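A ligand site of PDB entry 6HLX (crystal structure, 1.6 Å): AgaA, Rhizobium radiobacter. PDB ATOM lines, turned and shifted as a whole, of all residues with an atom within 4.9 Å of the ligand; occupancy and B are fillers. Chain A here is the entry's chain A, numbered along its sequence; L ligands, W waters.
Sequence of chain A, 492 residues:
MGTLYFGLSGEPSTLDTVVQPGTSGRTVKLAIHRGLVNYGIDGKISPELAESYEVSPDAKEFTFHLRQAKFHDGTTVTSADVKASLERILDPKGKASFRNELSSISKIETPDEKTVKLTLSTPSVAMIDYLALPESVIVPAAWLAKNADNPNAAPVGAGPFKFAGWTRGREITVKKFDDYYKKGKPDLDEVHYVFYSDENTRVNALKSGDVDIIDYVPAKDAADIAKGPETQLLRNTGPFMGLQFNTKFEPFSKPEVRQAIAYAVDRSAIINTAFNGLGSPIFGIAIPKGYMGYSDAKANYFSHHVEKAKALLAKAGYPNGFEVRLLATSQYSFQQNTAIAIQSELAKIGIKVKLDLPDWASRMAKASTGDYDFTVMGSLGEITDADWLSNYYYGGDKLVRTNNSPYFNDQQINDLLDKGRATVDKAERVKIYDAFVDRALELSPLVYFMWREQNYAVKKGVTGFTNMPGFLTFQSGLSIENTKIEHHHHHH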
ATOM      1  N   GLN A  20      13.269  24.808   8.094  1.00  0.00           N
ATOM      2  CA  GLN A  20      12.447  23.932   7.255  1.00  0.00           C
ATOM      3  C   GLN A  20      13.296  23.677   5.987  1.00  0.00           C
ATOM      4  O   GLN A  20      13.297  24.524   5.067  1.00  0.00           O
ATOM      5  CB  GLN A  20      11.122  24.652   6.891  1.00  0.00           C
ATOM      6  CG  GLN A  20       9.967  23.715   6.498  1.00  0.00           C
ATOM      7  CD  GLN A  20      10.286  22.722   5.416  1.00  0.00           C
ATOM      8  OE1 GLN A  20      11.069  21.780   5.616  1.00  0.00           O
ATOM      9  NE2 GLN A  20       9.656  22.869   4.258  1.00  0.00           N
ATOM     10  N   PRO A  21      14.081  22.585   5.917  1.00  0.00           N
ATOM     11  CA  PRO A  21      14.954  22.387   4.741  1.00  0.00           C
ATOM     12  C   PRO A  21      14.253  21.706   3.563  1.00  0.00           C
ATOM     13  O   PRO A  21      14.809  21.633   2.465  1.00  0.00           O
ATOM     14  CB  PRO A  21      16.047  21.444   5.281  1.00  0.00           C
ATOM     15  CG  PRO A  21      15.296  20.553   6.261  1.00  0.00           C
ATOM     16  CD  PRO A  21      14.220  21.465   6.897  1.00  0.00           C
ATOM     17  N   GLY A  22      13.093  21.141   3.837  1.00  0.00           N
ATOM     18  CA  GLY A  22      12.363  20.341   2.856  1.00  0.00           C
ATOM     19  C   GLY A  22      11.906  19.021   3.491  1.00  0.00           C
ATOM     20  O   GLY A  22      12.178  18.749   4.669  1.00  0.00           O
ATOM     21  N   THR A  23      11.194  18.210   2.709  1.00  0.00           N
ATOM     22  CA  THR A  23      10.596  16.956   3.199  1.00  0.00           C
ATOM     23  C   THR A  23      11.633  15.954   3.708  1.00  0.00           C
ATOM     24  O   THR A  23      11.348  15.243   4.686  1.00  0.00           O
ATOM     25  CB  THR A  23       9.694  16.372   2.109  1.00  0.00           C
ATOM     26  OG1 THR A  23       8.792  17.411   1.708  1.00  0.00           O
ATOM     27  CG2 THR A  23       8.903  15.150   2.569  1.00  0.00           C
ATOM     28  N   SER A  24      12.833  15.918   3.082  1.00  0.00           N
ATOM     29  CA  SER A  24      13.844  14.933   3.538  1.00  0.00           C
ATOM     30  C   SER A  24      14.262  15.174   4.996  1.00  0.00           C
ATOM     31  O   SER A  24      14.183  14.248   5.816  1.00  0.00           O
ATOM     32  CB  SER A  24      15.063  14.940   2.609  1.00  0.00           C
ATOM     33  OG  SER A  24      14.656  14.556   1.298  1.00  0.00           O
ATOM     34  N   ARG A  26      12.648  16.995   7.236  1.00  0.00           N
ATOM     35  CA  ARG A  26      11.472  16.825   8.092  1.00  0.00           C
ATOM     36  C   ARG A  26      11.230  15.362   8.448  1.00  0.00           C
ATOM     37  O   ARG A  26      10.908  15.060   9.593  1.00  0.00           O
ATOM     38  CB  ARG A  26      10.221  17.380   7.403  1.00  0.00           C
ATOM     39  CG  ARG A  26      10.225  18.891   7.426  1.00  0.00           C
ATOM     40  CD  ARG A  26       9.058  19.428   6.644  1.00  0.00           C
ATOM     41  NE  ARG A  26       8.531  20.598   7.336  1.00  0.00           N
ATOM     42  CZ  ARG A  26       7.461  21.286   6.933  1.00  0.00           C
ATOM     43  NH1 ARG A  26       6.853  20.978   5.793  1.00  0.00           N
ATOM     44  NH2 ARG A  26       7.010  22.300   7.670  1.00  0.00           N
ATOM     45  N   TYR A 216       8.664  10.241  -2.495  1.00  0.00           N
ATOM     46  CA  TYR A 216       8.636  10.916  -3.785  1.00  0.00           C
ATOM     47  C   TYR A 216       8.681   9.930  -4.962  1.00  0.00           C
ATOM     48  O   TYR A 216       9.568   9.989  -5.804  1.00  0.00           O
ATOM     49  CB  TYR A 216       9.772  11.945  -3.869  1.00  0.00           C
ATOM     50  CG  TYR A 216       9.476  13.231  -3.136  1.00  0.00           C
ATOM     51  CD1 TYR A 216       9.807  13.377  -1.791  1.00  0.00           C
ATOM     52  CD2 TYR A 216       8.952  14.334  -3.810  1.00  0.00           C
ATOM     53  CE1 TYR A 216       9.563  14.577  -1.112  1.00  0.00           C
ATOM     54  CE2 TYR A 216       8.710  15.543  -3.129  1.00  0.00           C
ATOM     55  CZ  TYR A 216       9.021  15.659  -1.780  1.00  0.00           C
ATOM     56  OH  TYR A 216       8.816  16.858  -1.116  1.00  0.00           O
ATOM     57  N   MET A 241       1.312  22.568  -7.379  1.00  0.00           N
ATOM     58  CA  MET A 241       2.422  23.176  -8.126  1.00  0.00           C
ATOM     59  C   MET A 241       1.985  24.579  -8.515  1.00  0.00           C
ATOM     60  O   MET A 241       0.861  24.775  -8.960  1.00  0.00           O
ATOM     61  CB  MET A 241       2.780  22.398  -9.416  1.00  0.00           C
ATOM     62  CG  MET A 241       3.292  20.985  -9.148  1.00  0.00           C
ATOM     63  SD  MET A 241       4.777  20.918  -8.124  1.00  0.00           S
ATOM     64  CE  MET A 241       5.949  21.693  -9.189  1.00  0.00           C
ATOM     65  N   GLN A 244       5.925  31.243  -6.823  1.00  0.00           N
ATOM     66  CA  GLN A 244       6.157  32.290  -5.822  1.00  0.00           C
ATOM     67  C   GLN A 244       6.962  33.350  -6.553  1.00  0.00           C
ATOM     68  O   GLN A 244       7.877  32.999  -7.313  1.00  0.00           O
ATOM     69  CB  GLN A 244       6.971  31.765  -4.619  1.00  0.00           C
ATOM     70  CG  GLN A 244       6.158  30.853  -3.730  1.00  0.00           C
ATOM     71  CD  GLN A 244       7.035  29.967  -2.901  1.00  0.00           C
ATOM     72  OE1 GLN A 244       7.148  28.778  -3.189  1.00  0.00           O
ATOM     73  NE2 GLN A 244       7.687  30.517  -1.874  1.00  0.00           N
ATOM     74  N   TYR A 332      14.618  17.019  -8.605  1.00  0.00           N
ATOM     75  CA  TYR A 332      13.283  16.431  -8.724  1.00  0.00           C
ATOM     76  C   TYR A 332      12.876  16.653 -10.169  1.00  0.00           C
ATOM     77  O   TYR A 332      12.700  17.811 -10.586  1.00  0.00           O
ATOM     78  CB  TYR A 332      12.326  17.124  -7.738  1.00  0.00           C
ATOM     79  CG  TYR A 332      12.719  16.853  -6.300  1.00  0.00           C
ATOM     80  CD1 TYR A 332      13.714  17.607  -5.676  1.00  0.00           C
ATOM     81  CD2 TYR A 332      12.142  15.800  -5.590  1.00  0.00           C
ATOM     82  CE1 TYR A 332      14.111  17.328  -4.372  1.00  0.00           C
ATOM     83  CE2 TYR A 332      12.544  15.509  -4.280  1.00  0.00           C
ATOM     84  CZ  TYR A 332      13.550  16.250  -3.694  1.00  0.00           C
ATOM     85  OH  TYR A 332      13.923  15.988  -2.405  1.00  0.00           O
ATOM     86  N   PHE A 334      10.165  16.348 -11.685  1.00  0.00           N
ATOM     87  CA  PHE A 334       8.922  17.132 -11.892  1.00  0.00           C
ATOM     88  C   PHE A 334       9.155  18.640 -11.766  1.00  0.00           C
ATOM     89  O   PHE A 334       8.473  19.407 -12.431  1.00  0.00           O
ATOM     90  CB  PHE A 334       7.781  16.638 -11.007  1.00  0.00           C
ATOM     91  CG  PHE A 334       7.954  16.906  -9.532  1.00  0.00           C
ATOM     92  CD1 PHE A 334       7.578  18.122  -8.971  1.00  0.00           C
ATOM     93  CD2 PHE A 334       8.502  15.935  -8.690  1.00  0.00           C
ATOM     94  CE1 PHE A 334       7.759  18.375  -7.608  1.00  0.00           C
ATOM     95  CE2 PHE A 334       8.665  16.178  -7.318  1.00  0.00           C
ATOM     96  CZ  PHE A 334       8.285  17.390  -6.781  1.00  0.00           C
ATOM     97  N   GLN A 335      10.095  19.061 -10.913  1.00  0.00           N
ATOM     98  CA  GLN A 335      10.395  20.495 -10.732  1.00  0.00           C
ATOM     99  C   GLN A 335      11.100  21.027 -11.995  1.00  0.00           C
ATOM    100  O   GLN A 335      10.702  22.065 -12.564  1.00  0.00           O
ATOM    101  CB  GLN A 335      11.305  20.682  -9.517  1.00  0.00           C
ATOM    102  CG  GLN A 335      10.602  20.494  -8.175  1.00  0.00           C
ATOM    103  CD  GLN A 335      10.485  21.791  -7.413  1.00  0.00           C
ATOM    104  OE1 GLN A 335      11.093  22.817  -7.746  1.00  0.00           O
ATOM    105  NE2 GLN A 335       9.695  21.770  -6.359  1.00  0.00           N
ATOM    106  N   TRP A 360      18.722  20.376  -4.665  1.00  0.00           N
ATOM    107  CA  TRP A 360      17.681  20.866  -3.779  1.00  0.00           C
ATOM    108  C   TRP A 360      18.194  21.804  -2.697  1.00  0.00           C
ATOM    109  O   TRP A 360      17.612  22.888  -2.494  1.00  0.00           O
ATOM    110  CB  TRP A 360      16.863  19.712  -3.161  1.00  0.00           C
ATOM    111  CG  TRP A 360      15.769  20.256  -2.294  1.00  0.00           C
ATOM    112  CD1 TRP A 360      15.747  20.289  -0.940  1.00  0.00           C
ATOM    113  CD2 TRP A 360      14.675  21.062  -2.741  1.00  0.00           C
ATOM    114  NE1 TRP A 360      14.632  20.965  -0.498  1.00  0.00           N
ATOM    115  CE2 TRP A 360      13.962  21.462  -1.584  1.00  0.00           C
ATOM    116  CE3 TRP A 360      14.184  21.434  -3.998  1.00  0.00           C
ATOM    117  CZ2 TRP A 360      12.803  22.232  -1.652  1.00  0.00           C
ATOM    118  CZ3 TRP A 360      13.025  22.194  -4.069  1.00  0.00           C
ATOM    119  CH2 TRP A 360      12.355  22.607  -2.900  1.00  0.00           C
ATOM    120  N   ARG A 363      18.889  25.211  -4.054  1.00  0.00           N
ATOM    121  CA  ARG A 363      17.635  25.936  -4.351  1.00  0.00           C
ATOM    122  C   ARG A 363      17.044  26.486  -3.025  1.00  0.00           C
ATOM    123  O   ARG A 363      16.641  27.645  -2.962  1.00  0.00           O
ATOM    124  CB  ARG A 363      16.614  24.965  -5.044  1.00  0.00           C
ATOM    125  CG  ARG A 363      15.233  25.565  -5.357  1.00  0.00           C
ATOM    126  CD  ARG A 363      14.289  25.538  -4.158  1.00  0.00           C
ATOM    127  NE  ARG A 363      13.000  26.127  -4.515  1.00  0.00           N
ATOM    128  CZ  ARG A 363      12.046  26.467  -3.653  1.00  0.00           C
ATOM    129  NH1 ARG A 363      10.927  27.037  -4.100  1.00  0.00           N
ATOM    130  NH2 ARG A 363      12.193  26.243  -2.355  1.00  0.00           N
ATOM    131  N   MET A 364      16.973  25.646  -1.976  1.00  0.00           N
ATOM    132  CA  MET A 364      16.398  26.054  -0.672  1.00  0.00           C
ATOM    133  C   MET A 364      17.174  27.196  -0.039  1.00  0.00           C
ATOM    134  O   MET A 364      16.547  28.072   0.558  1.00  0.00           O
ATOM    135  CB  MET A 364      16.357  24.885   0.344  1.00  0.00           C
ATOM    136  CG  MET A 364      15.100  24.108   0.358  1.00  0.00           C
ATOM    137  SD  MET A 364      13.547  25.064   0.367  1.00  0.00           S
ATOM    138  CE  MET A 364      13.088  25.082   2.002  1.00  0.00           C
ATOM    139  N   ALA A 367      16.062  30.209  -1.916  1.00  0.00           N
ATOM    140  CA  ALA A 367      14.656  30.507  -1.602  1.00  0.00           C
ATOM    141  C   ALA A 367      14.515  31.151  -0.219  1.00  0.00           C
ATOM    142  O   ALA A 367      13.734  32.102  -0.048  1.00  0.00           O
ATOM    143  CB  ALA A 367      13.806  29.239  -1.703  1.00  0.00           C
ATOM    144  N   VAL A 376       9.621  27.962  -8.872  1.00  0.00           N
ATOM    145  CA  VAL A 376       8.620  26.893  -8.948  1.00  0.00           C
ATOM    146  C   VAL A 376       8.273  26.532  -7.474  1.00  0.00           C
ATOM    147  O   VAL A 376       9.157  26.299  -6.641  1.00  0.00           O
ATOM    148  CB  VAL A 376       9.142  25.670  -9.719  1.00  0.00           C
ATOM    149  CG1 VAL A 376       8.212  24.461  -9.563  1.00  0.00           C
ATOM    150  CG2 VAL A 376       9.322  26.025 -11.205  1.00  0.00           C
ATOM    151  N   MET A 377       6.974  26.481  -7.190  1.00  0.00           N
ATOM    152  CA  MET A 377       6.471  26.193  -5.847  1.00  0.00           C
ATOM    153  C   MET A 377       5.814  24.816  -5.906  1.00  0.00           C
ATOM    154  O   MET A 377       4.870  24.631  -6.662  1.00  0.00           O
ATOM    155  CB  MET A 377       5.410  27.271  -5.457  1.00  0.00           C
ATOM    156  CG  MET A 377       4.603  26.958  -4.186  1.00  0.00           C
ATOM    157  SD  MET A 377       3.449  28.271  -3.738  1.00  0.00           S
ATOM    158  CE  MET A 377       2.244  28.215  -5.157  1.00  0.00           C
ATOM    159  N   GLY A 378       6.341  23.875  -5.128  1.00  0.00           N
ATOM    160  CA  GLY A 378       5.790  22.536  -4.943  1.00  0.00           C
ATOM    161  C   GLY A 378       5.511  22.454  -3.458  1.00  0.00           C
ATOM    162  O   GLY A 378       6.453  22.352  -2.673  1.00  0.00           O
ATOM    163  N   SER A 379       4.249  22.674  -3.031  1.00  0.00           N
ATOM    164  CA  SER A 379       4.025  22.836  -1.590  1.00  0.00           C
ATOM    165  C   SER A 379       2.613  22.546  -1.169  1.00  0.00           C
ATOM    166  O   SER A 379       1.847  21.953  -1.925  1.00  0.00           O
ATOM    167  CB  SER A 379       4.462  24.222  -1.129  1.00  0.00           C
ATOM    168  OG  SER A 379       4.753  24.214   0.269  1.00  0.00           O
ATOM    169  N   GLU A 382       0.733  24.295   5.537  1.00  0.00           N
ATOM    170  CA  GLU A 382       1.593  23.688   6.589  1.00  0.00           C
ATOM    171  C   GLU A 382       0.823  23.205   7.813  1.00  0.00           C
ATOM    172  O   GLU A 382       1.372  22.487   8.640  1.00  0.00           O
ATOM    173  CB  GLU A 382       2.710  24.651   6.981  1.00  0.00           C
ATOM    174  CG  GLU A 382       3.650  24.992   5.816  1.00  0.00           C
ATOM    175  CD  GLU A 382       4.610  23.902   5.367  1.00  0.00           C
ATOM    176  OE1 GLU A 382       4.627  22.781   5.962  1.00  0.00           O
ATOM    177  OE2 GLU A 382       5.333  24.161   4.392  1.00  0.00           O
ATOM    178  N   THR A 402       9.466  30.429   3.373  1.00  0.00           N
ATOM    179  CA  THR A 402       9.568  29.287   2.459  1.00  0.00           C
ATOM    180  C   THR A 402       8.411  29.195   1.440  1.00  0.00           C
ATOM    181  O   THR A 402       8.639  28.685   0.348  1.00  0.00           O
ATOM    182  CB  THR A 402       9.639  27.957   3.275  1.00  0.00           C
ATOM    183  OG1 THR A 402       8.466  27.866   4.105  1.00  0.00           O
ATOM    184  CG2 THR A 402      10.943  27.832   4.088  1.00  0.00           C
ATOM    185  N   ASN A 403       7.206  29.687   1.793  1.00  0.00           N
ATOM    186  CA  ASN A 403       5.986  29.532   0.975  1.00  0.00           C
ATOM    187  C   ASN A 403       5.397  30.812   0.410  1.00  0.00           C
ATOM    188  O   ASN A 403       4.414  30.720  -0.325  1.00  0.00           O
ATOM    189  CB  ASN A 403       4.900  28.828   1.800  1.00  0.00           C
ATOM    190  CG  ASN A 403       5.174  27.375   2.058  1.00  0.00           C
ATOM    191  OD1 ASN A 403       4.857  26.828   3.141  1.00  0.00           O
ATOM    192  ND2 ASN A 403       5.741  26.690   1.073  1.00  0.00           N
ATOM    193  N   ARG A 452      -1.072  17.788  -7.372  1.00  0.00           N
ATOM    194  CA  ARG A 452      -0.279  16.630  -7.802  1.00  0.00           C
ATOM    195  C   ARG A 452      -0.458  15.437  -6.863  1.00  0.00           C
ATOM    196  O   ARG A 452      -0.827  15.604  -5.700  1.00  0.00           O
ATOM    197  CB  ARG A 452       1.231  16.998  -7.884  1.00  0.00           C
ATOM    198  CG  ARG A 452       1.879  17.232  -6.517  1.00  0.00           C
ATOM    199  CD  ARG A 452       3.368  17.569  -6.632  1.00  0.00           C
ATOM    200  NE  ARG A 452       4.098  17.140  -5.438  1.00  0.00           N
ATOM    201  CZ  ARG A 452       5.037  17.852  -4.828  1.00  0.00           C
ATOM    202  NH1 ARG A 452       5.347  19.070  -5.278  1.00  0.00           N
ATOM    203  NH2 ARG A 452       5.687  17.368  -3.787  1.00  0.00           N
ATOM    204  N   PHE A 474       3.655  15.672   3.825  1.00  0.00           N
ATOM    205  CA  PHE A 474       5.078  15.904   4.115  1.00  0.00           C
ATOM    206  C   PHE A 474       5.476  15.554   5.573  1.00  0.00           C
ATOM    207  O   PHE A 474       6.674  15.558   5.894  1.00  0.00           O
ATOM    208  CB  PHE A 474       5.502  17.340   3.774  1.00  0.00           C
ATOM    209  CG  PHE A 474       5.460  17.729   2.305  1.00  0.00           C
ATOM    210  CD1 PHE A 474       5.386  16.756   1.307  1.00  0.00           C
ATOM    211  CD2 PHE A 474       5.561  19.060   1.929  1.00  0.00           C
ATOM    212  CE1 PHE A 474       5.389  17.131  -0.046  1.00  0.00           C
ATOM    213  CE2 PHE A 474       5.535  19.430   0.569  1.00  0.00           C
ATOM    214  CZ  PHE A 474       5.451  18.462  -0.407  1.00  0.00           C
HETATM  215  O1  LIG L   1      11.334  19.309  -0.008  1.00  0.00           O
HETATM  216  C1  LIG L   1      10.964  19.354  -1.184  1.00  0.00           C
HETATM  217  C2  LIG L   1      11.665  18.721  -2.235  1.00  0.00           C
HETATM  218  C3  LIG L   1      10.846  19.000  -3.532  1.00  0.00           C
HETATM  219  C4  LIG L   1       9.771  19.979  -3.116  1.00  0.00           C
HETATM  220  C5  LIG L   1       8.476  19.524  -3.537  1.00  0.00           C
HETATM  221  O2  LIG L   1       7.848  18.710  -2.797  1.00  0.00           O
HETATM  222  N1  LIG L   1       9.932  20.091  -1.635  1.00  0.00           N
HETATM  223  C6  LIG L   1       8.977  20.856  -0.728  1.00  0.00           C
HETATM  224  C7  LIG L   1       9.291  22.344  -0.768  1.00  0.00           C
HETATM  225  O3  LIG L   1       9.043  22.780  -2.112  1.00  0.00           O
HETATM  226  C8  LIG L   1       8.438  23.164   0.200  1.00  0.00           C
HETATM  227  O4  LIG L   1       8.370  22.455   1.471  1.00  0.00           O
HETATM  228  C9  LIG L   1       9.064  24.568   0.496  1.00  0.00           C
HETATM  229  O5  LIG L   1       8.230  25.284   1.415  1.00  0.00           O
HETATM  230  C10 LIG L   1       9.380  25.445  -0.741  1.00  0.00           C
HETATM  231  O6  LIG L   1      10.193  26.558  -0.336  1.00  0.00           O
HETATM  232  C11 LIG L   1       8.114  25.910  -1.476  1.00  0.00           C
HETATM  233  O7  LIG L   1       8.477  26.609  -2.692  1.00  0.00           O
HETATM  234  O8  LIG L   1       8.033  19.934  -4.636  1.00  0.00           O
HETATM  235  O   HOH W   1       8.524  19.954   3.252  1.00  0.00           O
HETATM  236  O   HOH W   2      13.613  17.795   0.866  1.00  0.00           O
HETATM  237  O   HOH W   3       7.832  25.172   4.058  1.00  0.00           O
HETATM  238  O   HOH W   4       5.760  22.571   2.249  1.00  0.00           O
HETATM  239  O   HOH W   5       9.211  24.215  -4.606  1.00  0.00           O
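Water W3 lies within hydrogen-bond range of O5 of the ligand (2.7 Å), OE2 of Glu 382 (2.7 Å), OG1 of Thr 402 (2.8 Å) and NE2 of Gln 20 (2.9 Å). Water W4 lies within hydrogen-bond range of the side-chain carboxylate (OE2) of Glu 382 (2.7 Å), an oxygen (O4) of the ligand (2.7 Å) and the side-chain hydroxyl (OG) of Ser 379 (2.8 Å). Water W2 lies within hydrogen-bond range of O1 of the ligand (2.9 Å), N of Ser 24 (3.0 Å) and N of Thr 23 (3.1 Å). Water W1 lies within hydrogen-bond range of the side-chain hydroxyl of Thr 23 (3.0 Å), an oxygen (O4) of the ligand (3.1 Å), the guanidinium group of Arg 26 (3.2 Å) and the side-chain amide nitrogen of Gln 20 (3.3 Å).
NE2 of Gln 244 sits at hydrogen-bond distance from O of Thr 402 (3.0 Å). The side-chain amide oxygen (OE1) of Gln 244 sits close to the side-chain sulfur (SD) of Met 377. The side-chain hydroxyl of Tyr 216 lies within hydrogen-bond range of the side-chain hydroxyl of Thr 23 (2.9 Å). SD of Met 241 sits at hydrogen-bond distance from NH1 of Arg 452. The side-chain sulfur (SD) of Met 364 sits at hydrogen-bond distance from the guanidinium group (NH2) of Arg 363. O of Val 376 is in hydrogen-bond range of NH1 of Arg 363, at 3.2 Å. The side-chain hydroxyl (OG) of Ser 379 is in hydrogen-bond range of the side-chain amide nitrogen (ND2) of Asn 403 (2.8 Å). The guanidinium group (NE) of Arg 26 sits close to the side-chain amide oxygen (OE1) of Gln 20.
The side-chain amide oxygen of Gln 244 sits at hydrogen-bond distance from an oxygen (O7) of the ligand (2.6 Å). An oxygen (O2) of the ligand lies within hydrogen-bond range of the side-chain hydroxyl (OH) of Tyr 216 (2.7 Å). O3 of the ligand lies within hydrogen-bond range of O of Gly 378 (2.7 Å). The backbone carbonyl oxygen (O) of Thr 402 sits at hydrogen-bond distance from an oxygen (O6) of the ligand (2.7 Å). NH2 of Arg 452 lies within salt-bridge range of O2 of the ligand (2.7 Å). The guanidinium group (NH1) of Arg 363 sits at hydrogen-bond distance from an oxygen (O7) of the ligand (2.9 Å). An oxygen (O5) of the ligand sits at hydrogen-bond distance from the side-chain amide nitrogen of Asn 403, 2.9 Å away. N of Thr 23 lies within hydrogen-bond range of O1 of the ligand, 2.9 Å away. The side-chain amide nitrogen (NE2) of Gln 335 sits at hydrogen-bond distance from an oxygen (O8) of the ligand, at 3.0 Å. The side-chain amide nitrogen of Gln 20 is in hydrogen-bond range of an oxygen (O4) of the ligand (3.1 Å). SD of Met 364 lies within hydrogen-bond range of O6 of the ligand, at 3.7 Å.
Gly 22 touches the ligand (CA to O1, 3.2 Å). Tyr 332 touches the ligand. Phe 334 touches the ligand. Trp 360 touches the ligand (CH2 to O3, 3.4 Å). CA of Met 377 touches O7 of the ligand, 3.8 Å away. OG of Ser 379 touches O5 of the ligand, 3.8 Å away. CZ of Phe 474 touches O2 of the ligand, 3.4 Å away. Hydrophobic or aromatic side chains within 4 Å of the ligand: Tyr 216, Tyr 332, Phe 334, Trp 360, Met 364 and Phe 474. The nearest printed residue that does not touch the ligand is Val 376 (4.02 Å).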
